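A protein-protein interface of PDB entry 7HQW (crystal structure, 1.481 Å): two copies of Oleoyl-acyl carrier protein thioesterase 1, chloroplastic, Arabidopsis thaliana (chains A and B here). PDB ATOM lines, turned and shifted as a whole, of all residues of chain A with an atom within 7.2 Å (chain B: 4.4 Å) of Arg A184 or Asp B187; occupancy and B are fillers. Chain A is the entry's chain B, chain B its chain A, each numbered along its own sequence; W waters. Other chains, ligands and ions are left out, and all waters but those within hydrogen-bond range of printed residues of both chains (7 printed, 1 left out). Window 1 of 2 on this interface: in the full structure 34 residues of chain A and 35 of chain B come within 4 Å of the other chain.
The side-chain carboxylate (OE1) of Glu B205 lies within hydrogen-bond range of the backbone NH (N) of Arg A185 (3.0 Å). The guanidinium group (NH1) of Arg B184 lies within salt-bridge range of the side-chain carboxylate (OE2) of Glu A31. N of Arg B185 lies within hydrogen-bond range of OE1 of Glu A205 (2.9 Å). NH2 of Arg B184 is in salt-bridge range of OD1 of Asp A187. NH1 of Arg A184 lies within salt-bridge range of OE2 of Glu B31 (2.8 Å). OD1 of Asp B187 lies within salt-bridge range of NH2 of Arg A184 (2.8 Å).
The backbone NH of Asn B195 sits at hydrogen-bond distance from the backbone carbonyl oxygen of Asp B187 (2.8 Å). OD1 of Asp A187 sits at hydrogen-bond distance from OG1 of Thr A198 (3.1 Å). The side-chain hydroxyl (OG1) of Thr B198 is in hydrogen-bond range of the side-chain carboxylate (OD1) of Asp B187. The backbone NH (N) of Arg A184 is in hydrogen-bond range of the side-chain carboxylate (OD2) of Asp A187, 2.9 Å away. N of Arg B184 sits at hydrogen-bond distance from OD2 of Asp B187 (2.9 Å).
Among the printed residues, pairs that only touch across the chains: Arg A184 with Glu B205 (3.5 Å), Glu A205 with Arg B184 (3.5 Å), Arg A184 with Gly B201 (3.7 Å), Thr A198 with Arg B184 (3.7 Å), Arg A184 with Thr B198 (3.8 Å), Glu A31 with Ala B186 (3.8 Å) and Ala A186 with Glu B31 (3.8 Å).
Arg A184 touches just these residues of chain B: Glu B31, Asp B187, Thr B198, Gly B201 and Glu B205. Of chain A, only Arg A184 (2.8 Å) comes within 4 Å of Asp B187. Of the printed residues of chain A, Arg B185 touches Glu A205 (2.9 Å). Of the printed residues of chain A, Glu B31 touches Arg A184 (2.8 Å) and Ala A186 (3.8 Å). Of the printed residues of chain B, Thr A198 touches Arg B184. Lys A182 touches none of the printed residues of chain B. Leu A188 touches none of the printed residues of chain B. The nearest residue of chain B that does not touch Arg A184 is Trp B202 (4.1 Å). The nearest printed residue of chain A that does not touch Thr B198 is Ala A186 (7.8 Å).
Of the 15 printed residues of chain B, 8 touch a printed residue of chain A. Hydrophobic or aromatic side chains of chain B that line the printed part of chain A: Ala B186. Hydrophobic or aromatic side chains of chain A that line the printed part of chain B: Ala A186. Among the printed residues, Asp or Glu carboxylates within 4 Å of a Lys or Arg side-chain nitrogen of the other chain: Glu A31 with Arg B184 (2.8 Å), Arg A184 with Glu B31 (2.8 Å), Arg A184 with Asp B187 (2.8 Å) and Asp A187 with Arg B184 (2.8 Å).
Glu A31 touches Ala B186, and with the chains exchanged Ala A186 touches Glu B31. Arg A184 touches Asp B187, and with the chains exchanged Asp A187 touches Arg B184. Arg A184 touches Thr B198, and with the chains exchanged Thr A198 touches Arg B184. Arg A184 touches Glu B205, and with the chains exchanged Glu A205 touches Arg B184. Positions printed for both chains: 31, 183, 184, 185, 186, 187, 188, 194, 198, 202 and 205.
Water W5 bridges OE2 of Glu B31 (2.6 Å) and NH2 of Arg A184 (2.9 Å). Water W3 bridges OD2 of Asp B187 (2.6 Å) and NE of Arg A184 (2.8 Å). Water W4 bridges the side-chain carboxylate (OE2) of Glu A31 and the guanidinium group (NH2) of Arg B184. Water W2 lies within hydrogen-bond range of the side-chain carboxylate (OE1) of Glu A31 (2.7 Å), the guanidinium group (NH1) of Arg B184 (2.9 Å) and the backbone NH (N) of Ala B186 (2.9 Å). Water W6 lies within hydrogen-bond range of the side-chain carboxylate of Glu A205 (2.9 Å) and the backbone carbonyl oxygen of Pro B183 (3.0 Å). Water W1 lies within hydrogen-bond range of OE2 of Glu B205 and O of Pro A183.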
ATOM      1  N   GLU A  31      15.490   4.195  -4.947  1.00  0.00           N
ATOM      2  CA  GLU A  31      15.475   2.799  -5.396  1.00  0.00           C
ATOM      3  C   GLU A  31      16.770   2.484  -6.168  1.00  0.00           C
ATOM      4  O   GLU A  31      17.345   1.409  -5.972  1.00  0.00           O
ATOM      5  CB  GLU A  31      14.239   2.489  -6.260  1.00  0.00           C
ATOM      6  CG  GLU A  31      12.981   2.513  -5.410  1.00  0.00           C
ATOM      7  CD  GLU A  31      11.736   2.198  -6.213  1.00  0.00           C
ATOM      8  OE1 GLU A  31      10.986   3.148  -6.551  1.00  0.00           O
ATOM      9  OE2 GLU A  31      11.513   0.994  -6.482  1.00  0.00           O
ATOM     10  N   LYS A 182       1.038  -4.900  -7.720  1.00  0.00           N
ATOM     11  CA  LYS A 182       1.480  -6.276  -7.924  1.00  0.00           C
ATOM     12  C   LYS A 182       2.801  -6.318  -8.691  1.00  0.00           C
ATOM     13  O   LYS A 182       3.070  -5.455  -9.535  1.00  0.00           O
ATOM     14  CB  LYS A 182       0.430  -7.138  -8.610  1.00  0.00           C
ATOM     15  CG  LYS A 182       0.052  -6.705  -9.992  1.00  0.00           C
ATOM     16  CD  LYS A 182      -1.154  -7.543 -10.440  1.00  0.00           C
ATOM     17  CE  LYS A 182      -1.532  -7.296 -11.886  1.00  0.00           C
ATOM     18  NZ  LYS A 182      -2.867  -7.883 -12.206  1.00  0.00           N
ATOM     19  N   PRO A 183       3.651  -7.287  -8.359  1.00  0.00           N
ATOM     20  CA  PRO A 183       4.956  -7.357  -9.030  1.00  0.00           C
ATOM     21  C   PRO A 183       4.865  -7.894 -10.460  1.00  0.00           C
ATOM     22  O   PRO A 183       4.015  -8.729 -10.774  1.00  0.00           O
ATOM     23  CB  PRO A 183       5.766  -8.332  -8.140  1.00  0.00           C
ATOM     24  CG  PRO A 183       4.719  -9.250  -7.562  1.00  0.00           C
ATOM     25  CD  PRO A 183       3.494  -8.360  -7.345  1.00  0.00           C
ATOM     26  N   ARG A 184       5.769  -7.428 -11.334  1.00  0.00           N
ATOM     27  CA  ARG A 184       5.894  -7.991 -12.672  1.00  0.00           C
ATOM     28  C   ARG A 184       7.271  -8.745 -12.717  1.00  0.00           C
ATOM     29  O   ARG A 184       8.015  -8.689 -11.733  1.00  0.00           O
ATOM     30  CB  ARG A 184       5.756  -6.924 -13.781  1.00  0.00           C
ATOM     31  CG  ARG A 184       6.689  -5.718 -13.688  1.00  0.00           C
ATOM     32  CD  ARG A 184       6.237  -4.689 -14.737  1.00  0.00           C
ATOM     33  NE  ARG A 184       7.059  -3.471 -14.781  1.00  0.00           N
ATOM     34  CZ  ARG A 184       8.118  -3.314 -15.574  1.00  0.00           C
ATOM     35  NH1 ARG A 184       8.563  -4.330 -16.313  1.00  0.00           N
ATOM     36  NH2 ARG A 184       8.767  -2.154 -15.602  1.00  0.00           N
ATOM     37  N   ARG A 185       7.618  -9.415 -13.822  1.00  0.00           N
ATOM     38  CA  ARG A 185       8.867 -10.199 -13.858  1.00  0.00           C
ATOM     39  C   ARG A 185      10.100  -9.379 -13.564  1.00  0.00           C
ATOM     40  O   ARG A 185      11.012  -9.886 -12.918  1.00  0.00           O
ATOM     41  CB  ARG A 185       9.039 -10.990 -15.168  1.00  0.00           C
ATOM     42  CG  ARG A 185       7.998 -12.093 -15.317  1.00  0.00           C
ATOM     43  CD  ARG A 185       8.472 -13.276 -16.149  1.00  0.00           C
ATOM     44  NE  ARG A 185       7.315 -14.123 -16.447  1.00  0.00           N
ATOM     45  CZ  ARG A 185       6.555 -14.001 -17.528  1.00  0.00           C
ATOM     46  NH1 ARG A 185       6.862 -13.118 -18.469  1.00  0.00           N
ATOM     47  NH2 ARG A 185       5.506 -14.788 -17.698  1.00  0.00           N
ATOM     48  N   ALA A 186      10.118  -8.090 -13.979  1.00  0.00           N
ATOM     49  CA  ALA A 186      11.286  -7.227 -13.697  1.00  0.00           C
ATOM     50  C   ALA A 186      11.494  -6.996 -12.202  1.00  0.00           C
ATOM     51  O   ALA A 186      12.585  -6.621 -11.795  1.00  0.00           O
ATOM     52  CB  ALA A 186      11.114  -5.875 -14.385  1.00  0.00           C
ATOM     53  N   ASP A 187      10.449  -7.161 -11.396  1.00  0.00           N
ATOM     54  CA  ASP A 187      10.575  -6.985  -9.934  1.00  0.00           C
ATOM     55  C   ASP A 187      11.171  -8.237  -9.240  1.00  0.00           C
ATOM     56  O   ASP A 187      11.403  -8.185  -8.037  1.00  0.00           O
ATOM     57  CB  ASP A 187       9.194  -6.736  -9.315  1.00  0.00           C
ATOM     58  CG  ASP A 187       8.618  -5.384  -9.713  1.00  0.00           C
ATOM     59  OD1 ASP A 187       9.292  -4.373  -9.477  1.00  0.00           O
ATOM     60  OD2 ASP A 187       7.467  -5.352 -10.243  1.00  0.00           O
ATOM     61  N   LEU A 188      11.343  -9.329  -9.951  1.00  0.00           N
ATOM     62  CA  LEU A 188      11.856 -10.570  -9.352  1.00  0.00           C
ATOM     63  C   LEU A 188      13.364 -10.669  -9.481  1.00  0.00           C
ATOM     64  O   LEU A 188      13.960 -10.053 -10.378  1.00  0.00           O
ATOM     65  CB  LEU A 188      11.213 -11.788 -10.022  1.00  0.00           C
ATOM     66  CG  LEU A 188       9.685 -11.792 -10.075  1.00  0.00           C
ATOM     67  CD1 LEU A 188       9.181 -13.020 -10.799  1.00  0.00           C
ATOM     68  CD2 LEU A 188       9.057 -11.610  -8.643  1.00  0.00           C
ATOM     69  N   VAL A 194      10.429 -11.692  -5.030  1.00  0.00           N
ATOM     70  CA  VAL A 194      10.352 -10.226  -5.202  1.00  0.00           C
ATOM     71  C   VAL A 194      11.634  -9.573  -4.608  1.00  0.00           C
ATOM     72  O   VAL A 194      12.076  -9.913  -3.494  1.00  0.00           O
ATOM     73  CB  VAL A 194       9.059  -9.627  -4.574  1.00  0.00           C
ATOM     74  CG1 VAL A 194       9.068  -8.099  -4.636  1.00  0.00           C
ATOM     75  CG2 VAL A 194       7.802 -10.210  -5.260  1.00  0.00           C
ATOM     76  N   THR A 198      11.850  -3.546  -4.480  1.00  0.00           N
ATOM     77  CA  THR A 198      10.463  -3.355  -4.922  1.00  0.00           C
ATOM     78  C   THR A 198       9.570  -2.876  -3.781  1.00  0.00           C
ATOM     79  O   THR A 198       8.783  -1.944  -3.971  1.00  0.00           O
ATOM     80  CB  THR A 198       9.933  -4.651  -5.571  1.00  0.00           C
ATOM     81  OG1 THR A 198      10.729  -4.925  -6.745  1.00  0.00           O
ATOM     82  CG2 THR A 198       8.458  -4.535  -5.970  1.00  0.00           C
ATOM     83  N   TRP A 202       7.035   0.293  -3.448  1.00  0.00           N
ATOM     84  CA  TRP A 202       5.616   0.177  -3.006  1.00  0.00           C
ATOM     85  C   TRP A 202       5.294   1.065  -1.814  1.00  0.00           C
ATOM     86  O   TRP A 202       4.219   1.667  -1.779  1.00  0.00           O
ATOM     87  CB  TRP A 202       5.238  -1.268  -2.739  1.00  0.00           C
ATOM     88  CG  TRP A 202       5.130  -2.132  -3.972  1.00  0.00           C
ATOM     89  CD1 TRP A 202       4.901  -1.735  -5.260  1.00  0.00           C
ATOM     90  CD2 TRP A 202       5.234  -3.556  -3.998  1.00  0.00           C
ATOM     91  NE1 TRP A 202       4.833  -2.835  -6.085  1.00  0.00           N
ATOM     92  CE2 TRP A 202       5.040  -3.970  -5.333  1.00  0.00           C
ATOM     93  CE3 TRP A 202       5.538  -4.516  -3.024  1.00  0.00           C
ATOM     94  CZ2 TRP A 202       5.073  -5.323  -5.707  1.00  0.00           C
ATOM     95  CZ3 TRP A 202       5.653  -5.843  -3.404  1.00  0.00           C
ATOM     96  CH2 TRP A 202       5.390  -6.241  -4.732  1.00  0.00           C
ATOM     97  N   GLU A 205       4.830   4.623  -3.099  1.00  0.00           N
ATOM     98  CA  GLU A 205       3.691   4.888  -3.983  1.00  0.00           C
ATOM     99  C   GLU A 205       2.539   5.631  -3.294  1.00  0.00           C
ATOM    100  O   GLU A 205       1.752   6.283  -3.977  1.00  0.00           O
ATOM    101  CB  GLU A 205       3.117   3.586  -4.558  1.00  0.00           C
ATOM    102  CG  GLU A 205       3.799   3.098  -5.826  1.00  0.00           C
ATOM    103  CD  GLU A 205       3.799   4.116  -6.953  1.00  0.00           C
ATOM    104  OE1 GLU A 205       4.845   4.771  -7.161  1.00  0.00           O
ATOM    105  OE2 GLU A 205       2.762   4.241  -7.643  1.00  0.00           O
ATOM    106  N   GLN A 230       5.032 -13.920  -5.784  1.00  0.00           N
ATOM    107  CA  GLN A 230       4.870 -13.418  -7.161  1.00  0.00           C
ATOM    108  C   GLN A 230       3.377 -13.295  -7.584  1.00  0.00           C
ATOM    109  O   GLN A 230       3.058 -12.484  -8.454  1.00  0.00           O
ATOM    110  CB  GLN A 230       5.650 -14.313  -8.151  1.00  0.00           C
ATOM    111  CG  GLN A 230       5.815 -13.693  -9.529  1.00  0.00           C
ATOM    112  CD  GLN A 230       6.047 -14.705 -10.636  1.00  0.00           C
ATOM    113  OE1 GLN A 230       5.755 -14.434 -11.813  1.00  0.00           O
ATOM    114  NE2 GLN A 230       6.586 -15.886 -10.301  1.00  0.00           N
ATOM    115  N   GLU B  31      14.681  -6.636 -20.834  1.00  0.00           N
ATOM    116  CA  GLU B  31      14.424  -5.267 -20.346  1.00  0.00           C
ATOM    117  C   GLU B  31      15.758  -4.619 -19.948  1.00  0.00           C
ATOM    118  O   GLU B  31      15.978  -3.439 -20.261  1.00  0.00           O
ATOM    119  CB  GLU B  31      13.433  -5.250 -19.165  1.00  0.00           C
ATOM    120  CG  GLU B  31      12.044  -5.620 -19.657  1.00  0.00           C
ATOM    121  CD  GLU B  31      11.017  -5.600 -18.546  1.00  0.00           C
ATOM    122  OE1 GLU B  31      10.633  -6.699 -18.060  1.00  0.00           O
ATOM    123  OE2 GLU B  31      10.600  -4.476 -18.178  1.00  0.00           O
ATOM    124  N   PRO B 183       1.711   1.676 -13.965  1.00  0.00           N
ATOM    125  CA  PRO B 183       3.091   2.083 -13.675  1.00  0.00           C
ATOM    126  C   PRO B 183       3.258   2.632 -12.254  1.00  0.00           C
ATOM    127  O   PRO B 183       2.334   3.241 -11.689  1.00  0.00           O
ATOM    128  CB  PRO B 183       3.359   3.190 -14.728  1.00  0.00           C
ATOM    129  CG  PRO B 183       2.012   3.796 -14.958  1.00  0.00           C
ATOM    130  CD  PRO B 183       1.031   2.634 -14.869  1.00  0.00           C
ATOM    131  N   ARG B 184       4.449   2.429 -11.680  1.00  0.00           N
ATOM    132  CA  ARG B 184       4.791   3.054 -10.403  1.00  0.00           C
ATOM    133  C   ARG B 184       5.880   4.119 -10.702  1.00  0.00           C
ATOM    134  O   ARG B 184       6.321   4.215 -11.852  1.00  0.00           O
ATOM    135  CB  ARG B 184       5.208   2.017  -9.336  1.00  0.00           C
ATOM    136  CG  ARG B 184       6.359   1.086  -9.707  1.00  0.00           C
ATOM    137  CD  ARG B 184       6.479   0.024  -8.594  1.00  0.00           C
ATOM    138  NE  ARG B 184       7.542  -0.972  -8.817  1.00  0.00           N
ATOM    139  CZ  ARG B 184       8.794  -0.835  -8.373  1.00  0.00           C
ATOM    140  NH1 ARG B 184       9.173   0.287  -7.760  1.00  0.00           N
ATOM    141  NH2 ARG B 184       9.681  -1.812  -8.550  1.00  0.00           N
ATOM    142  N   ARG B 185       6.344   4.898  -9.698  1.00  0.00           N
ATOM    143  CA  ARG B 185       7.306   5.965  -9.982  1.00  0.00           C
ATOM    144  C   ARG B 185       8.582   5.466 -10.620  1.00  0.00           C
ATOM    145  O   ARG B 185       9.133   6.161 -11.471  1.00  0.00           O
ATOM    146  CB  ARG B 185       7.637   6.803  -8.736  1.00  0.00           C
ATOM    147  CG  ARG B 185       6.453   7.656  -8.288  1.00  0.00           C
ATOM    148  CD  ARG B 185       6.872   8.946  -7.564  1.00  0.00           C
ATOM    149  NE  ARG B 185       5.692   9.534  -6.940  1.00  0.00           N
ATOM    150  CZ  ARG B 185       5.267   9.246  -5.712  1.00  0.00           C
ATOM    151  NH1 ARG B 185       5.973   8.434  -4.928  1.00  0.00           N
ATOM    152  NH2 ARG B 185       4.155   9.794  -5.243  1.00  0.00           N
ATOM    153  N   ALA B 186       9.025   4.234 -10.278  1.00  0.00           N
ATOM    154  CA  ALA B 186      10.257   3.687 -10.887  1.00  0.00           C
ATOM    155  C   ALA B 186      10.114   3.471 -12.397  1.00  0.00           C
ATOM    156  O   ALA B 186      11.121   3.381 -13.092  1.00  0.00           O
ATOM    157  CB  ALA B 186      10.627   2.362 -10.226  1.00  0.00           C
ATOM    158  N   ASP B 187       8.886   3.339 -12.883  1.00  0.00           N
ATOM    159  CA  ASP B 187       8.642   3.158 -14.327  1.00  0.00           C
ATOM    160  C   ASP B 187       8.701   4.476 -15.112  1.00  0.00           C
ATOM    161  O   ASP B 187       8.588   4.440 -16.335  1.00  0.00           O
ATOM    162  CB  ASP B 187       7.261   2.543 -14.565  1.00  0.00           C
ATOM    163  CG  ASP B 187       7.165   1.103 -14.079  1.00  0.00           C
ATOM    164  OD1 ASP B 187       7.999   0.279 -14.518  1.00  0.00           O
ATOM    165  OD2 ASP B 187       6.242   0.802 -13.246  1.00  0.00           O
ATOM    166  N   LEU B 188       8.791   5.609 -14.441  1.00  0.00           N
ATOM    167  CA  LEU B 188       8.792   6.911 -15.116  1.00  0.00           C
ATOM    168  C   LEU B 188      10.204   7.391 -15.391  1.00  0.00           C
ATOM    169  O   LEU B 188      11.129   7.011 -14.681  1.00  0.00           O
ATOM    170  CB  LEU B 188       8.079   7.958 -14.253  1.00  0.00           C
ATOM    171  CG  LEU B 188       6.670   7.579 -13.783  1.00  0.00           C
ATOM    172  CD1 LEU B 188       6.084   8.670 -12.907  1.00  0.00           C
ATOM    173  CD2 LEU B 188       5.739   7.194 -14.995  1.00  0.00           C
ATOM    174  N   ASP B 189      10.365   8.270 -16.399  1.00  0.00           N
ATOM    175  CA  ASP B 189      11.647   8.902 -16.701  1.00  0.00           C
ATOM    176  C   ASP B 189      11.739  10.271 -15.971  1.00  0.00           C
ATOM    177  O   ASP B 189      10.827  10.641 -15.228  1.00  0.00           O
ATOM    178  CB  ASP B 189      11.836   9.032 -18.230  1.00  0.00           C
ATOM    179  CG  ASP B 189      10.831   9.946 -18.919  1.00  0.00           C
ATOM    180  OD1 ASP B 189      10.103  10.672 -18.212  1.00  0.00           O
ATOM    181  OD2 ASP B 189      10.773   9.933 -20.170  1.00  0.00           O
ATOM    182  N   HIS B 193       7.240  10.712 -17.679  1.00  0.00           N
ATOM    183  CA  HIS B 193       6.566   9.920 -18.709  1.00  0.00           C
ATOM    184  C   HIS B 193       6.930   8.428 -18.488  1.00  0.00           C
ATOM    185  O   HIS B 193       8.036   8.147 -18.023  1.00  0.00           O
ATOM    186  CB  HIS B 193       7.003  10.362 -20.106  1.00  0.00           C
ATOM    187  CG  HIS B 193       6.363  11.657 -20.540  1.00  0.00           C
ATOM    188  ND1 HIS B 193       5.226  11.675 -21.338  1.00  0.00           N
ATOM    189  CD2 HIS B 193       6.672  12.933 -20.197  1.00  0.00           C
ATOM    190  CE1 HIS B 193       4.911  12.953 -21.484  1.00  0.00           C
ATOM    191  NE2 HIS B 193       5.743  13.745 -20.802  1.00  0.00           N
ATOM    192  N   VAL B 194       6.035   7.490 -18.857  1.00  0.00           N
ATOM    193  CA  VAL B 194       6.359   6.063 -18.715  1.00  0.00           C
ATOM    194  C   VAL B 194       7.551   5.724 -19.649  1.00  0.00           C
ATOM    195  O   VAL B 194       7.581   6.136 -20.835  1.00  0.00           O
ATOM    196  CB  VAL B 194       5.137   5.143 -18.989  1.00  0.00           C
ATOM    197  CG1 VAL B 194       5.543   3.659 -18.983  1.00  0.00           C
ATOM    198  CG2 VAL B 194       4.013   5.404 -17.975  1.00  0.00           C
ATOM    199  N   ASN B 195       8.577   5.073 -19.087  1.00  0.00           N
ATOM    200  CA  ASN B 195       9.771   4.704 -19.849  1.00  0.00           C
ATOM    201  C   ASN B 195       9.369   3.686 -20.937  1.00  0.00           C
ATOM    202  O   ASN B 195       8.578   2.777 -20.670  1.00  0.00           O
ATOM    203  CB  ASN B 195      10.793   4.052 -18.914  1.00  0.00           C
ATOM    204  CG  ASN B 195      12.159   3.857 -19.562  1.00  0.00           C
ATOM    205  OD1 ASN B 195      12.331   3.184 -20.604  1.00  0.00           O
ATOM    206  ND2 ASN B 195      13.177   4.438 -18.974  1.00  0.00           N
ATOM    207  N   THR B 198       9.220  -0.063 -20.051  1.00  0.00           N
ATOM    208  CA  THR B 198       8.103  -0.573 -19.242  1.00  0.00           C
ATOM    209  C   THR B 198       7.087  -1.298 -20.116  1.00  0.00           C
ATOM    210  O   THR B 198       6.654  -2.389 -19.753  1.00  0.00           O
ATOM    211  CB  THR B 198       7.460   0.577 -18.437  1.00  0.00           C
ATOM    212  OG1 THR B 198       8.447   1.081 -17.510  1.00  0.00           O
ATOM    213  CG2 THR B 198       6.228   0.110 -17.661  1.00  0.00           C
ATOM    214  N   GLY B 201       8.117  -4.803 -20.795  1.00  0.00           N
ATOM    215  CA  GLY B 201       7.784  -5.637 -19.638  1.00  0.00           C
ATOM    216  C   GLY B 201       6.296  -5.992 -19.604  1.00  0.00           C
ATOM    217  O   GLY B 201       5.953  -7.159 -19.447  1.00  0.00           O
ATOM    218  N   TRP B 202       5.426  -5.006 -19.877  1.00  0.00           N
ATOM    219  CA  TRP B 202       3.964  -5.264 -19.902  1.00  0.00           C
ATOM    220  C   TRP B 202       3.553  -6.247 -20.995  1.00  0.00           C
ATOM    221  O   TRP B 202       2.697  -7.102 -20.761  1.00  0.00           O
ATOM    222  CB  TRP B 202       3.181  -3.971 -20.004  1.00  0.00           C
ATOM    223  CG  TRP B 202       3.206  -3.118 -18.768  1.00  0.00           C
ATOM    224  CD1 TRP B 202       3.411  -3.514 -17.481  1.00  0.00           C
ATOM    225  CD2 TRP B 202       2.935  -1.710 -18.724  1.00  0.00           C
ATOM    226  NE1 TRP B 202       3.318  -2.424 -16.633  1.00  0.00           N
ATOM    227  CE2 TRP B 202       3.024  -1.304 -17.373  1.00  0.00           C
ATOM    228  CE3 TRP B 202       2.718  -0.741 -19.712  1.00  0.00           C
ATOM    229  CZ2 TRP B 202       2.804   0.030 -16.976  1.00  0.00           C
ATOM    230  CZ3 TRP B 202       2.604   0.585 -19.331  1.00  0.00           C
ATOM    231  CH2 TRP B 202       2.624   0.956 -17.967  1.00  0.00           C
ATOM    232  N   GLU B 205       4.341  -9.748 -19.762  1.00  0.00           N
ATOM    233  CA  GLU B 205       3.585 -10.256 -18.602  1.00  0.00           C
ATOM    234  C   GLU B 205       2.516 -11.282 -18.985  1.00  0.00           C
ATOM    235  O   GLU B 205       2.132 -12.082 -18.140  1.00  0.00           O
ATOM    236  CB  GLU B 205       2.888  -9.114 -17.855  1.00  0.00           C
ATOM    237  CG  GLU B 205       3.741  -8.435 -16.790  1.00  0.00           C
ATOM    238  CD  GLU B 205       4.300  -9.385 -15.748  1.00  0.00           C
ATOM    239  OE1 GLU B 205       5.497  -9.737 -15.857  1.00  0.00           O
ATOM    240  OE2 GLU B 205       3.552  -9.773 -14.820  1.00  0.00           O
HETATM  241  O   HOH W   1       2.064  -8.027 -12.932  1.00  0.00           O
HETATM  242  O   HOH W   2       8.530   3.136  -7.591  1.00  0.00           O
HETATM  243  O   HOH W   3       5.920  -1.772 -12.843  1.00  0.00           O
HETATM  244  O   HOH W   4      12.357  -1.018  -7.980  1.00  0.00           O
HETATM  245  O   HOH W   5      11.268  -2.252 -16.978  1.00  0.00           O
HETATM  246  O   HOH W   6       1.336   2.155  -9.120  1.00  0.00           O
HETATM  247  O   HOH W   7       6.394  -2.969 -10.451  1.00  0.00           O
